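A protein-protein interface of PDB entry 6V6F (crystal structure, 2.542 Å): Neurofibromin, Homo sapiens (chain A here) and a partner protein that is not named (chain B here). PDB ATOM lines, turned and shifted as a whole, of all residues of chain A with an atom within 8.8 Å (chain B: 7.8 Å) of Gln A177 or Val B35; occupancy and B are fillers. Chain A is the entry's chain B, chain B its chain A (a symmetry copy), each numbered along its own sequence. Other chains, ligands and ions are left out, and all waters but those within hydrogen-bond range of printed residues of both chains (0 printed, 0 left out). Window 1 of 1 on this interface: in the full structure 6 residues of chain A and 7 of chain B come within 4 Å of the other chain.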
ATOM      1  N   MET A  70      -6.523   0.497 -10.369  1.00  0.00           N
ATOM      2  CA  MET A  70      -7.137   1.688 -10.941  1.00  0.00           C
ATOM      3  C   MET A  70      -6.419   2.154 -12.202  1.00  0.00           C
ATOM      4  O   MET A  70      -7.022   2.857 -13.022  1.00  0.00           O
ATOM      5  CB  MET A  70      -7.163   2.811  -9.903  1.00  0.00           C
ATOM      6  CG  MET A  70      -7.960   4.027 -10.330  1.00  0.00           C
ATOM      7  SD  MET A  70      -7.766   5.436  -9.228  1.00  0.00           S
ATOM      8  CE  MET A  70      -8.563   6.701 -10.210  1.00  0.00           C
ATOM      9  N   TYR A 168     -17.363   9.327 -12.643  1.00  0.00           N
ATOM     10  CA  TYR A 168     -16.650   9.780 -11.454  1.00  0.00           C
ATOM     11  C   TYR A 168     -17.207   9.136 -10.190  1.00  0.00           C
ATOM     12  O   TYR A 168     -16.450   8.809  -9.269  1.00  0.00           O
ATOM     13  CB  TYR A 168     -16.724  11.305 -11.368  1.00  0.00           C
ATOM     14  CG  TYR A 168     -16.126  11.900 -10.117  1.00  0.00           C
ATOM     15  CD1 TYR A 168     -14.816  11.626  -9.750  1.00  0.00           C
ATOM     16  CD2 TYR A 168     -16.867  12.756  -9.314  1.00  0.00           C
ATOM     17  CE1 TYR A 168     -14.264  12.177  -8.608  1.00  0.00           C
ATOM     18  CE2 TYR A 168     -16.324  13.313  -8.171  1.00  0.00           C
ATOM     19  CZ  TYR A 168     -15.023  13.019  -7.824  1.00  0.00           C
ATOM     20  OH  TYR A 168     -14.478  13.573  -6.685  1.00  0.00           O
ATOM     21  N   VAL A 171     -16.336   5.045 -10.093  1.00  0.00           N
ATOM     22  CA  VAL A 171     -14.960   4.762  -9.700  1.00  0.00           C
ATOM     23  C   VAL A 171     -14.727   5.136  -8.242  1.00  0.00           C
ATOM     24  O   VAL A 171     -13.961   4.467  -7.535  1.00  0.00           O
ATOM     25  CB  VAL A 171     -13.982   5.493 -10.639  1.00  0.00           C
ATOM     26  CG1 VAL A 171     -12.544   5.314 -10.174  1.00  0.00           C
ATOM     27  CG2 VAL A 171     -14.149   4.993 -12.067  1.00  0.00           C
ATOM     28  N   SER A 172     -15.393   6.188  -7.760  1.00  0.00           N
ATOM     29  CA  SER A 172     -15.179   6.651  -6.393  1.00  0.00           C
ATOM     30  C   SER A 172     -15.612   5.629  -5.351  1.00  0.00           C
ATOM     31  O   SER A 172     -15.143   5.692  -4.209  1.00  0.00           O
ATOM     32  CB  SER A 172     -15.921   7.970  -6.166  1.00  0.00           C
ATOM     33  OG  SER A 172     -15.415   8.989  -7.010  1.00  0.00           O
ATOM     34  N   GLN A 173     -16.487   4.692  -5.708  1.00  0.00           N
ATOM     35  CA  GLN A 173     -16.952   3.691  -4.756  1.00  0.00           C
ATOM     36  C   GLN A 173     -15.956   2.557  -4.543  1.00  0.00           C
ATOM     37  O   GLN A 173     -16.233   1.657  -3.742  1.00  0.00           O
ATOM     38  CB  GLN A 173     -18.303   3.127  -5.202  1.00  0.00           C
ATOM     39  CG  GLN A 173     -19.438   4.133  -5.105  1.00  0.00           C
ATOM     40  CD  GLN A 173     -19.518   4.788  -3.737  1.00  0.00           C
ATOM     41  OE1 GLN A 173     -19.207   5.969  -3.582  1.00  0.00           O
ATOM     42  NE2 GLN A 173     -19.933   4.020  -2.736  1.00  0.00           N
ATOM     43  N   ARG A 174     -14.816   2.571  -5.233  1.00  0.00           N
ATOM     44  CA  ARG A 174     -13.735   1.635  -4.957  1.00  0.00           C
ATOM     45  C   ARG A 174     -12.360   2.281  -4.911  1.00  0.00           C
ATOM     46  O   ARG A 174     -11.452   1.704  -4.298  1.00  0.00           O
ATOM     47  CB  ARG A 174     -13.710   0.502  -5.995  1.00  0.00           C
ATOM     48  CG  ARG A 174     -13.331  -0.850  -5.402  1.00  0.00           C
ATOM     49  CD  ARG A 174     -13.109  -1.915  -6.466  1.00  0.00           C
ATOM     50  NE  ARG A 174     -11.704  -2.020  -6.851  1.00  0.00           N
ATOM     51  CZ  ARG A 174     -11.191  -3.032  -7.544  1.00  0.00           C
ATOM     52  NH1 ARG A 174      -9.901  -3.044  -7.847  1.00  0.00           N
ATOM     53  NH2 ARG A 174     -11.968  -4.036  -7.929  1.00  0.00           N
ATOM     54  N   PHE A 175     -12.170   3.445  -5.527  1.00  0.00           N
ATOM     55  CA  PHE A 175     -10.912   4.188  -5.475  1.00  0.00           C
ATOM     56  C   PHE A 175     -11.246   5.623  -5.095  1.00  0.00           C
ATOM     57  O   PHE A 175     -11.331   6.503  -5.961  1.00  0.00           O
ATOM     58  CB  PHE A 175     -10.168   4.121  -6.810  1.00  0.00           C
ATOM     59  CG  PHE A 175     -10.044   2.730  -7.366  1.00  0.00           C
ATOM     60  CD1 PHE A 175      -9.051   1.877  -6.916  1.00  0.00           C
ATOM     61  CD2 PHE A 175     -10.918   2.279  -8.341  1.00  0.00           C
ATOM     62  CE1 PHE A 175      -8.933   0.598  -7.425  1.00  0.00           C
ATOM     63  CE2 PHE A 175     -10.806   1.000  -8.855  1.00  0.00           C
ATOM     64  CZ  PHE A 175      -9.812   0.159  -8.396  1.00  0.00           C
ATOM     65  N   PRO A 176     -11.450   5.894  -3.802  1.00  0.00           N
ATOM     66  CA  PRO A 176     -11.876   7.249  -3.414  1.00  0.00           C
ATOM     67  C   PRO A 176     -10.828   8.313  -3.682  1.00  0.00           C
ATOM     68  O   PRO A 176     -11.183   9.448  -4.024  1.00  0.00           O
ATOM     69  CB  PRO A 176     -12.174   7.104  -1.914  1.00  0.00           C
ATOM     70  CG  PRO A 176     -11.331   5.953  -1.475  1.00  0.00           C
ATOM     71  CD  PRO A 176     -11.307   5.002  -2.639  1.00  0.00           C
ATOM     72  N   GLN A 177      -9.547   7.984  -3.545  1.00  0.00           N
ATOM     73  CA  GLN A 177      -8.489   8.972  -3.720  1.00  0.00           C
ATOM     74  C   GLN A 177      -8.187   9.160  -5.202  1.00  0.00           C
ATOM     75  O   GLN A 177      -7.822   8.203  -5.894  1.00  0.00           O
ATOM     76  CB  GLN A 177      -7.232   8.554  -2.962  1.00  0.00           C
ATOM     77  CG  GLN A 177      -7.369   8.610  -1.446  1.00  0.00           C
ATOM     78  CD  GLN A 177      -7.528  10.026  -0.918  1.00  0.00           C
ATOM     79  OE1 GLN A 177      -7.321  11.002  -1.640  1.00  0.00           O
ATOM     80  NE2 GLN A 177      -7.896  10.143   0.353  1.00  0.00           N
ATOM     81  N   ASN A 178      -8.345  10.396  -5.679  1.00  0.00           N
ATOM     82  CA  ASN A 178      -7.986  10.776  -7.045  1.00  0.00           C
ATOM     83  C   ASN A 178      -8.775   9.981  -8.084  1.00  0.00           C
ATOM     84  O   ASN A 178      -8.266   9.653  -9.156  1.00  0.00           O
ATOM     85  CB  ASN A 178      -6.480  10.631  -7.281  1.00  0.00           C
ATOM     86  CG  ASN A 178      -5.678  11.712  -6.589  1.00  0.00           C
ATOM     87  OD1 ASN A 178      -5.456  12.786  -7.146  1.00  0.00           O
ATOM     88  ND2 ASN A 178      -5.237  11.434  -5.368  1.00  0.00           N
ATOM     89  N   SER A 179     -10.037   9.677  -7.767  1.00  0.00           N
ATOM     90  CA  SER A 179     -10.912   9.046  -8.747  1.00  0.00           C
ATOM     91  C   SER A 179     -11.161   9.947  -9.949  1.00  0.00           C
ATOM     92  O   SER A 179     -11.566   9.456 -11.007  1.00  0.00           O
ATOM     93  CB  SER A 179     -12.240   8.656  -8.095  1.00  0.00           C
ATOM     94  OG  SER A 179     -12.795   9.739  -7.370  1.00  0.00           O
ATOM     95  N   ILE A 180     -10.923  11.253  -9.805  1.00  0.00           N
ATOM     96  CA  ILE A 180     -11.041  12.179 -10.922  1.00  0.00           C
ATOM     97  C   ILE A 180      -9.978  11.916 -11.983  1.00  0.00           C
ATOM     98  O   ILE A 180     -10.142  12.327 -13.138  1.00  0.00           O
ATOM     99  CB  ILE A 180     -10.965  13.627 -10.394  1.00  0.00           C
ATOM    100  CG1 ILE A 180     -11.300  14.636 -11.495  1.00  0.00           C
ATOM    101  CG2 ILE A 180      -9.595  13.911  -9.801  1.00  0.00           C
ATOM    102  CD1 ILE A 180     -12.703  14.507 -12.023  1.00  0.00           C
ATOM    103  N   GLY A 181      -8.893  11.226 -11.625  1.00  0.00           N
ATOM    104  CA  GLY A 181      -7.839  10.969 -12.593  1.00  0.00           C
ATOM    105  C   GLY A 181      -8.278  10.057 -13.721  1.00  0.00           C
ATOM    106  O   GLY A 181      -7.888  10.253 -14.875  1.00  0.00           O
ATOM    107  N   ALA A 182      -9.095   9.048 -13.408  1.00  0.00           N
ATOM    108  CA  ALA A 182      -9.579   8.140 -14.443  1.00  0.00           C
ATOM    109  C   ALA A 182     -10.566   8.825 -15.377  1.00  0.00           C
ATOM    110  O   ALA A 182     -10.691   8.431 -16.543  1.00  0.00           O
ATOM    111  CB  ALA A 182     -10.220   6.908 -13.805  1.00  0.00           C
ATOM    112  N   ARG A 254      -6.794  19.041 -13.867  1.00  0.00           N
ATOM    113  CA  ARG A 254      -7.688  18.511 -12.842  1.00  0.00           C
ATOM    114  C   ARG A 254      -8.811  19.491 -12.521  1.00  0.00           C
ATOM    115  O   ARG A 254      -9.958  19.079 -12.318  1.00  0.00           O
ATOM    116  CB  ARG A 254      -6.900  18.171 -11.577  1.00  0.00           C
ATOM    117  CG  ARG A 254      -5.977  16.974 -11.722  1.00  0.00           C
ATOM    118  CD  ARG A 254      -5.213  16.722 -10.436  1.00  0.00           C
ATOM    119  NE  ARG A 254      -6.105  16.597  -9.286  1.00  0.00           N
ATOM    120  CZ  ARG A 254      -6.575  15.442  -8.829  1.00  0.00           C
ATOM    121  NH1 ARG A 254      -7.382  15.422  -7.777  1.00  0.00           N
ATOM    122  NH2 ARG A 254      -6.239  14.305  -9.422  1.00  0.00           N
ATOM    123  N   TYR B   2      -3.838  19.955   8.774  1.00  0.00           N
ATOM    124  CA  TYR B   2      -3.454  21.338   9.030  1.00  0.00           C
ATOM    125  C   TYR B   2      -4.180  21.925  10.235  1.00  0.00           C
ATOM    126  O   TYR B   2      -3.708  22.914  10.805  1.00  0.00           O
ATOM    127  CB  TYR B   2      -3.715  22.196   7.791  1.00  0.00           C
ATOM    128  CG  TYR B   2      -2.787  21.912   6.629  1.00  0.00           C
ATOM    129  CD1 TYR B   2      -2.986  20.811   5.805  1.00  0.00           C
ATOM    130  CD2 TYR B   2      -1.717  22.753   6.349  1.00  0.00           C
ATOM    131  CE1 TYR B   2      -2.141  20.551   4.740  1.00  0.00           C
ATOM    132  CE2 TYR B   2      -0.867  22.502   5.288  1.00  0.00           C
ATOM    133  CZ  TYR B   2      -1.084  21.400   4.486  1.00  0.00           C
ATOM    134  OH  TYR B   2      -0.241  21.148   3.428  1.00  0.00           O
ATOM    135  N   PHE B  33      -7.115  19.098   5.598  1.00  0.00           N
ATOM    136  CA  PHE B  33      -6.044  18.162   5.293  1.00  0.00           C
ATOM    137  C   PHE B  33      -5.785  18.157   3.795  1.00  0.00           C
ATOM    138  O   PHE B  33      -6.548  18.719   3.005  1.00  0.00           O
ATOM    139  CB  PHE B  33      -6.382  16.750   5.783  1.00  0.00           C
ATOM    140  CG  PHE B  33      -7.686  16.220   5.251  1.00  0.00           C
ATOM    141  CD1 PHE B  33      -8.874  16.478   5.914  1.00  0.00           C
ATOM    142  CD2 PHE B  33      -7.725  15.464   4.089  1.00  0.00           C
ATOM    143  CE1 PHE B  33     -10.075  15.994   5.430  1.00  0.00           C
ATOM    144  CE2 PHE B  33      -8.923  14.978   3.600  1.00  0.00           C
ATOM    145  CZ  PHE B  33     -10.099  15.243   4.272  1.00  0.00           C
ATOM    146  N   LYS B  34      -4.691  17.506   3.411  1.00  0.00           N
ATOM    147  CA  LYS B  34      -4.324  17.338   2.015  1.00  0.00           C
ATOM    148  C   LYS B  34      -4.281  15.857   1.666  1.00  0.00           C
ATOM    149  O   LYS B  34      -3.944  15.012   2.503  1.00  0.00           O
ATOM    150  CB  LYS B  34      -2.962  17.982   1.702  1.00  0.00           C
ATOM    151  CG  LYS B  34      -1.757  17.213   2.235  1.00  0.00           C
ATOM    152  CD  LYS B  34      -0.450  17.757   1.675  1.00  0.00           C
ATOM    153  CE  LYS B  34       0.733  16.885   2.074  1.00  0.00           C
ATOM    154  NZ  LYS B  34       2.019  17.384   1.509  1.00  0.00           N
ATOM    155  N   VAL B  35      -4.646  15.549   0.428  1.00  0.00           N
ATOM    156  CA  VAL B  35      -4.453  14.228  -0.151  1.00  0.00           C
ATOM    157  C   VAL B  35      -3.634  14.412  -1.421  1.00  0.00           C
ATOM    158  O   VAL B  35      -4.028  15.171  -2.312  1.00  0.00           O
ATOM    159  CB  VAL B  35      -5.781  13.506  -0.436  1.00  0.00           C
ATOM    160  CG1 VAL B  35      -6.458  13.125   0.873  1.00  0.00           C
ATOM    161  CG2 VAL B  35      -6.712  14.367  -1.267  1.00  0.00           C
ATOM    162  N   PRO B  36      -2.476  13.772  -1.543  1.00  0.00           N
ATOM    163  CA  PRO B  36      -1.549  14.121  -2.620  1.00  0.00           C
ATOM    164  C   PRO B  36      -1.893  13.455  -3.942  1.00  0.00           C
ATOM    165  O   PRO B  36      -2.408  12.336  -3.993  1.00  0.00           O
ATOM    166  CB  PRO B  36      -0.204  13.615  -2.091  1.00  0.00           C
ATOM    167  CG  PRO B  36      -0.578  12.447  -1.241  1.00  0.00           C
ATOM    168  CD  PRO B  36      -1.898  12.794  -0.606  1.00  0.00           C
ATOM    169  N   HIS B  37      -1.602  14.175  -5.023  1.00  0.00           N
ATOM    170  CA  HIS B  37      -1.598  13.577  -6.351  1.00  0.00           C
ATOM    171  C   HIS B  37      -0.311  12.775  -6.499  1.00  0.00           C
ATOM    172  O   HIS B  37       0.785  13.341  -6.419  1.00  0.00           O
ATOM    173  CB  HIS B  37      -1.688  14.645  -7.442  1.00  0.00           C
ATOM    174  CG  HIS B  37      -2.714  15.706  -7.186  1.00  0.00           C
ATOM    175  ND1 HIS B  37      -2.707  16.914  -7.850  1.00  0.00           N
ATOM    176  CD2 HIS B  37      -3.780  15.745  -6.351  1.00  0.00           C
ATOM    177  CE1 HIS B  37      -3.718  17.653  -7.431  1.00  0.00           C
ATOM    178  NE2 HIS B  37      -4.385  16.966  -6.520  1.00  0.00           N
ATOM    179  N   GLN B  38      -0.428  11.472  -6.721  1.00  0.00           N
ATOM    180  CA  GLN B  38       0.810  10.666  -6.890  1.00  0.00           C
ATOM    181  C   GLN B  38       1.646  10.669  -5.606  1.00  0.00           C
ATOM    182  O   GLN B  38       1.146  10.190  -4.585  1.00  0.00           O
ATOM    183  CB  GLN B  38       1.630  11.208  -8.059  1.00  0.00           C
ATOM    184  CG  GLN B  38       0.916  11.118  -9.396  1.00  0.00           C
ATOM    185  CD  GLN B  38       0.401   9.733  -9.700  1.00  0.00           C
ATOM    186  OE1 GLN B  38       0.493   8.821  -8.886  1.00  0.00           O
ATOM    187  NE2 GLN B  38      -0.157   9.566 -10.887  1.00  0.00           N
ATOM    188  N   GLU B  39       2.893  11.141  -5.693  1.00  0.00           N
ATOM    189  CA  GLU B  39       3.864  11.160  -4.566  1.00  0.00           C
ATOM    190  C   GLU B  39       3.333  12.009  -3.404  1.00  0.00           C
ATOM    191  O   GLU B  39       2.845  13.115  -3.657  1.00  0.00           O
ATOM    192  CB  GLU B  39       5.198  11.690  -5.085  1.00  0.00           C
ATOM    193  CG  GLU B  39       5.062  13.012  -5.812  1.00  0.00           C
ATOM    194  CD  GLU B  39       4.791  12.912  -7.299  1.00  0.00           C
ATOM    195  OE1 GLU B  39       4.151  13.834  -7.845  1.00  0.00           O
ATOM    196  OE2 GLU B  39       5.243  11.924  -7.907  1.00  0.00           O
ATOM    197  N   GLU B  40       3.525  11.523  -2.173  1.00  0.00           N
ATOM    198  CA  GLU B  40       2.973  12.134  -0.966  1.00  0.00           C
ATOM    199  C   GLU B  40       3.470  13.564  -0.787  1.00  0.00           C
ATOM    200  O   GLU B  40       2.679  14.478  -0.523  1.00  0.00           O
ATOM    201  CB  GLU B  40       3.326  11.282   0.254  1.00  0.00           C
ATOM    202  CG  GLU B  40       2.993   9.805   0.092  1.00  0.00           C
ATOM    203  CD  GLU B  40       1.501   9.546   0.013  1.00  0.00           C
ATOM    204  OE1 GLU B  40       0.735  10.271   0.683  1.00  0.00           O
ATOM    205  OE2 GLU B  40       1.094   8.618  -0.718  1.00  0.00           O
ATOM    206  N   GLY B  42       4.170  15.972  -2.710  1.00  0.00           N
ATOM    207  CA  GLY B  42       4.003  16.691  -3.958  1.00  0.00           C
ATOM    208  C   GLY B  42       2.688  17.439  -4.028  1.00  0.00           C
ATOM    209  O   GLY B  42       2.107  17.776  -2.992  1.00  0.00           O
ATOM    210  N   CYS B  43       2.207  17.703  -5.242  1.00  0.00           N
ATOM    211  CA  CYS B  43       0.947  18.413  -5.417  1.00  0.00           C
ATOM    212  C   CYS B  43      -0.207  17.616  -4.818  1.00  0.00           C
ATOM    213  O   CYS B  43      -0.179  16.384  -4.763  1.00  0.00           O
ATOM    214  CB  CYS B  43       0.693  18.682  -6.899  1.00  0.00           C
ATOM    215  SG  CYS B  43       0.921  17.236  -7.959  1.00  0.00           S
ATOM    216  N   ALA B  44      -1.237  18.334  -4.371  1.00  0.00           N
ATOM    217  CA  ALA B  44      -2.308  17.716  -3.605  1.00  0.00           C
ATOM    218  C   ALA B  44      -3.594  18.516  -3.760  1.00  0.00           C
ATOM    219  O   ALA B  44      -3.599  19.639  -4.269  1.00  0.00           O
ATOM    220  CB  ALA B  44      -1.932  17.605  -2.123  1.00  0.00           C
ATOM    221  N   ASP B  45      -4.691  17.909  -3.318  1.00  0.00           N
ATOM    222  CA  ASP B  45      -5.960  18.591  -3.115  1.00  0.00           C
ATOM    223  C   ASP B  45      -6.161  18.834  -1.625  1.00  0.00           C
ATOM    224  O   ASP B  45      -5.702  18.055  -0.787  1.00  0.00           O
ATOM    225  CB  ASP B  45      -7.131  17.775  -3.668  1.00  0.00           C
ATOM    226  CG  ASP B  45      -7.059  17.587  -5.170  1.00  0.00           C
ATOM    227  OD1 ASP B  45      -6.587  18.508  -5.867  1.00  0.00           O
ATOM    228  OD2 ASP B  45      -7.478  16.514  -5.653  1.00  0.00           O
ATOM    229  N   PHE B  46      -6.854  19.921  -1.299  1.00  0.00           N
ATOM    230  CA  PHE B  46      -7.075  20.318   0.084  1.00  0.00           C
ATOM    231  C   PHE B  46      -8.570  20.388   0.364  1.00  0.00           C
ATOM    232  O   PHE B  46      -9.352  20.803  -0.497  1.00  0.00           O
ATOM    233  CB  PHE B  46      -6.400  21.662   0.381  1.00  0.00           C
ATOM    234  CG  PHE B  46      -4.898  21.616   0.289  1.00  0.00           C
ATOM    235  CD1 PHE B  46      -4.262  21.669  -0.943  1.00  0.00           C
ATOM    236  CD2 PHE B  46      -4.123  21.512   1.431  1.00  0.00           C
ATOM    237  CE1 PHE B  46      -2.882  21.622  -1.030  1.00  0.00           C
ATOM    238  CE2 PHE B  46      -2.742  21.467   1.350  1.00  0.00           C
ATOM    239  CZ  PHE B  46      -2.121  21.520   0.117  1.00  0.00           C
ATOM    240  N   PHE B  47      -8.964  19.974   1.567  1.00  0.00           N
ATOM    241  CA  PHE B  47     -10.375  19.829   1.893  1.00  0.00           C
ATOM    242  C   PHE B  47     -10.660  20.323   3.302  1.00  0.00           C
ATOM    243  O   PHE B  47      -9.769  20.418   4.149  1.00  0.00           O
ATOM    244  CB  PHE B  47     -10.840  18.371   1.773  1.00  0.00           C
ATOM    245  CG  PHE B  47     -10.646  17.779   0.411  1.00  0.00           C
ATOM    246  CD1 PHE B  47     -11.632  17.890  -0.554  1.00  0.00           C
ATOM    247  CD2 PHE B  47      -9.480  17.106   0.097  1.00  0.00           C
ATOM    248  CE1 PHE B  47     -11.455  17.343  -1.811  1.00  0.00           C
ATOM    249  CE2 PHE B  47      -9.301  16.558  -1.156  1.00  0.00           C
ATOM    250  CZ  PHE B  47     -10.288  16.676  -2.110  1.00  0.00           C
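The backbone carbonyl oxygen (O) of Pro B36 lies within hydrogen-bond range of the side-chain amide nitrogen (ND2) of Asn A178, at 3.3 Å. A ring nitrogen (NE2) of His B37 sits close to the guanidinium group of Arg A254, 3.3 Å away. The side-chain carboxylate (OD1) of Asp B45 lies within salt-bridge range of the guanidinium group (NH1) of Arg A254 (3.7 Å).
No residue of chain B comes within 4 Å of Pro A176. Of chain B, only Val B35 (3.2 Å) comes within 4 Å of Gln A177. Printed residues of chain B within 4 Å of Asn A178: Pro B36 (3.3 Å) and His B37 (3.5 Å). Of the printed residues of chain B, Arg A254 touches His B37 and Asp B45. Of chain A, only Gln A177 comes within 4 Å of Val B35. Of chain A, only Asn A178 (3.3 Å) comes within 4 Å of Pro B36. Of the printed residues of chain A, His B37 touches Asn A178 (3.5 Å) and Arg A254 (3.2 Å). Glu B40 touches none of the printed residues of chain A. Of the printed residues of chain A, Asp B45 touches Arg A254.
Among the printed residues, merely in contact across the chains: Gln A177 with Val B35 and Asn A178 with His B37.
The backbone carbonyl oxygen (O) of Asp B45 lies within hydrogen-bond range of the backbone NH (N) of Val B35 (3.0 Å). NE2 of His B37 lies within hydrogen-bond range of OD1 of Asp B45 (2.8 Å). The side-chain amide oxygen (OD1) of Asn A178 is in hydrogen-bond range of the guanidinium group (NH2) of Arg A254 (2.8 Å).
Of the 15 printed residues of chain B, 4 touch a printed residue of chain A. Among the printed residues, 5 pairs touch across the chains.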
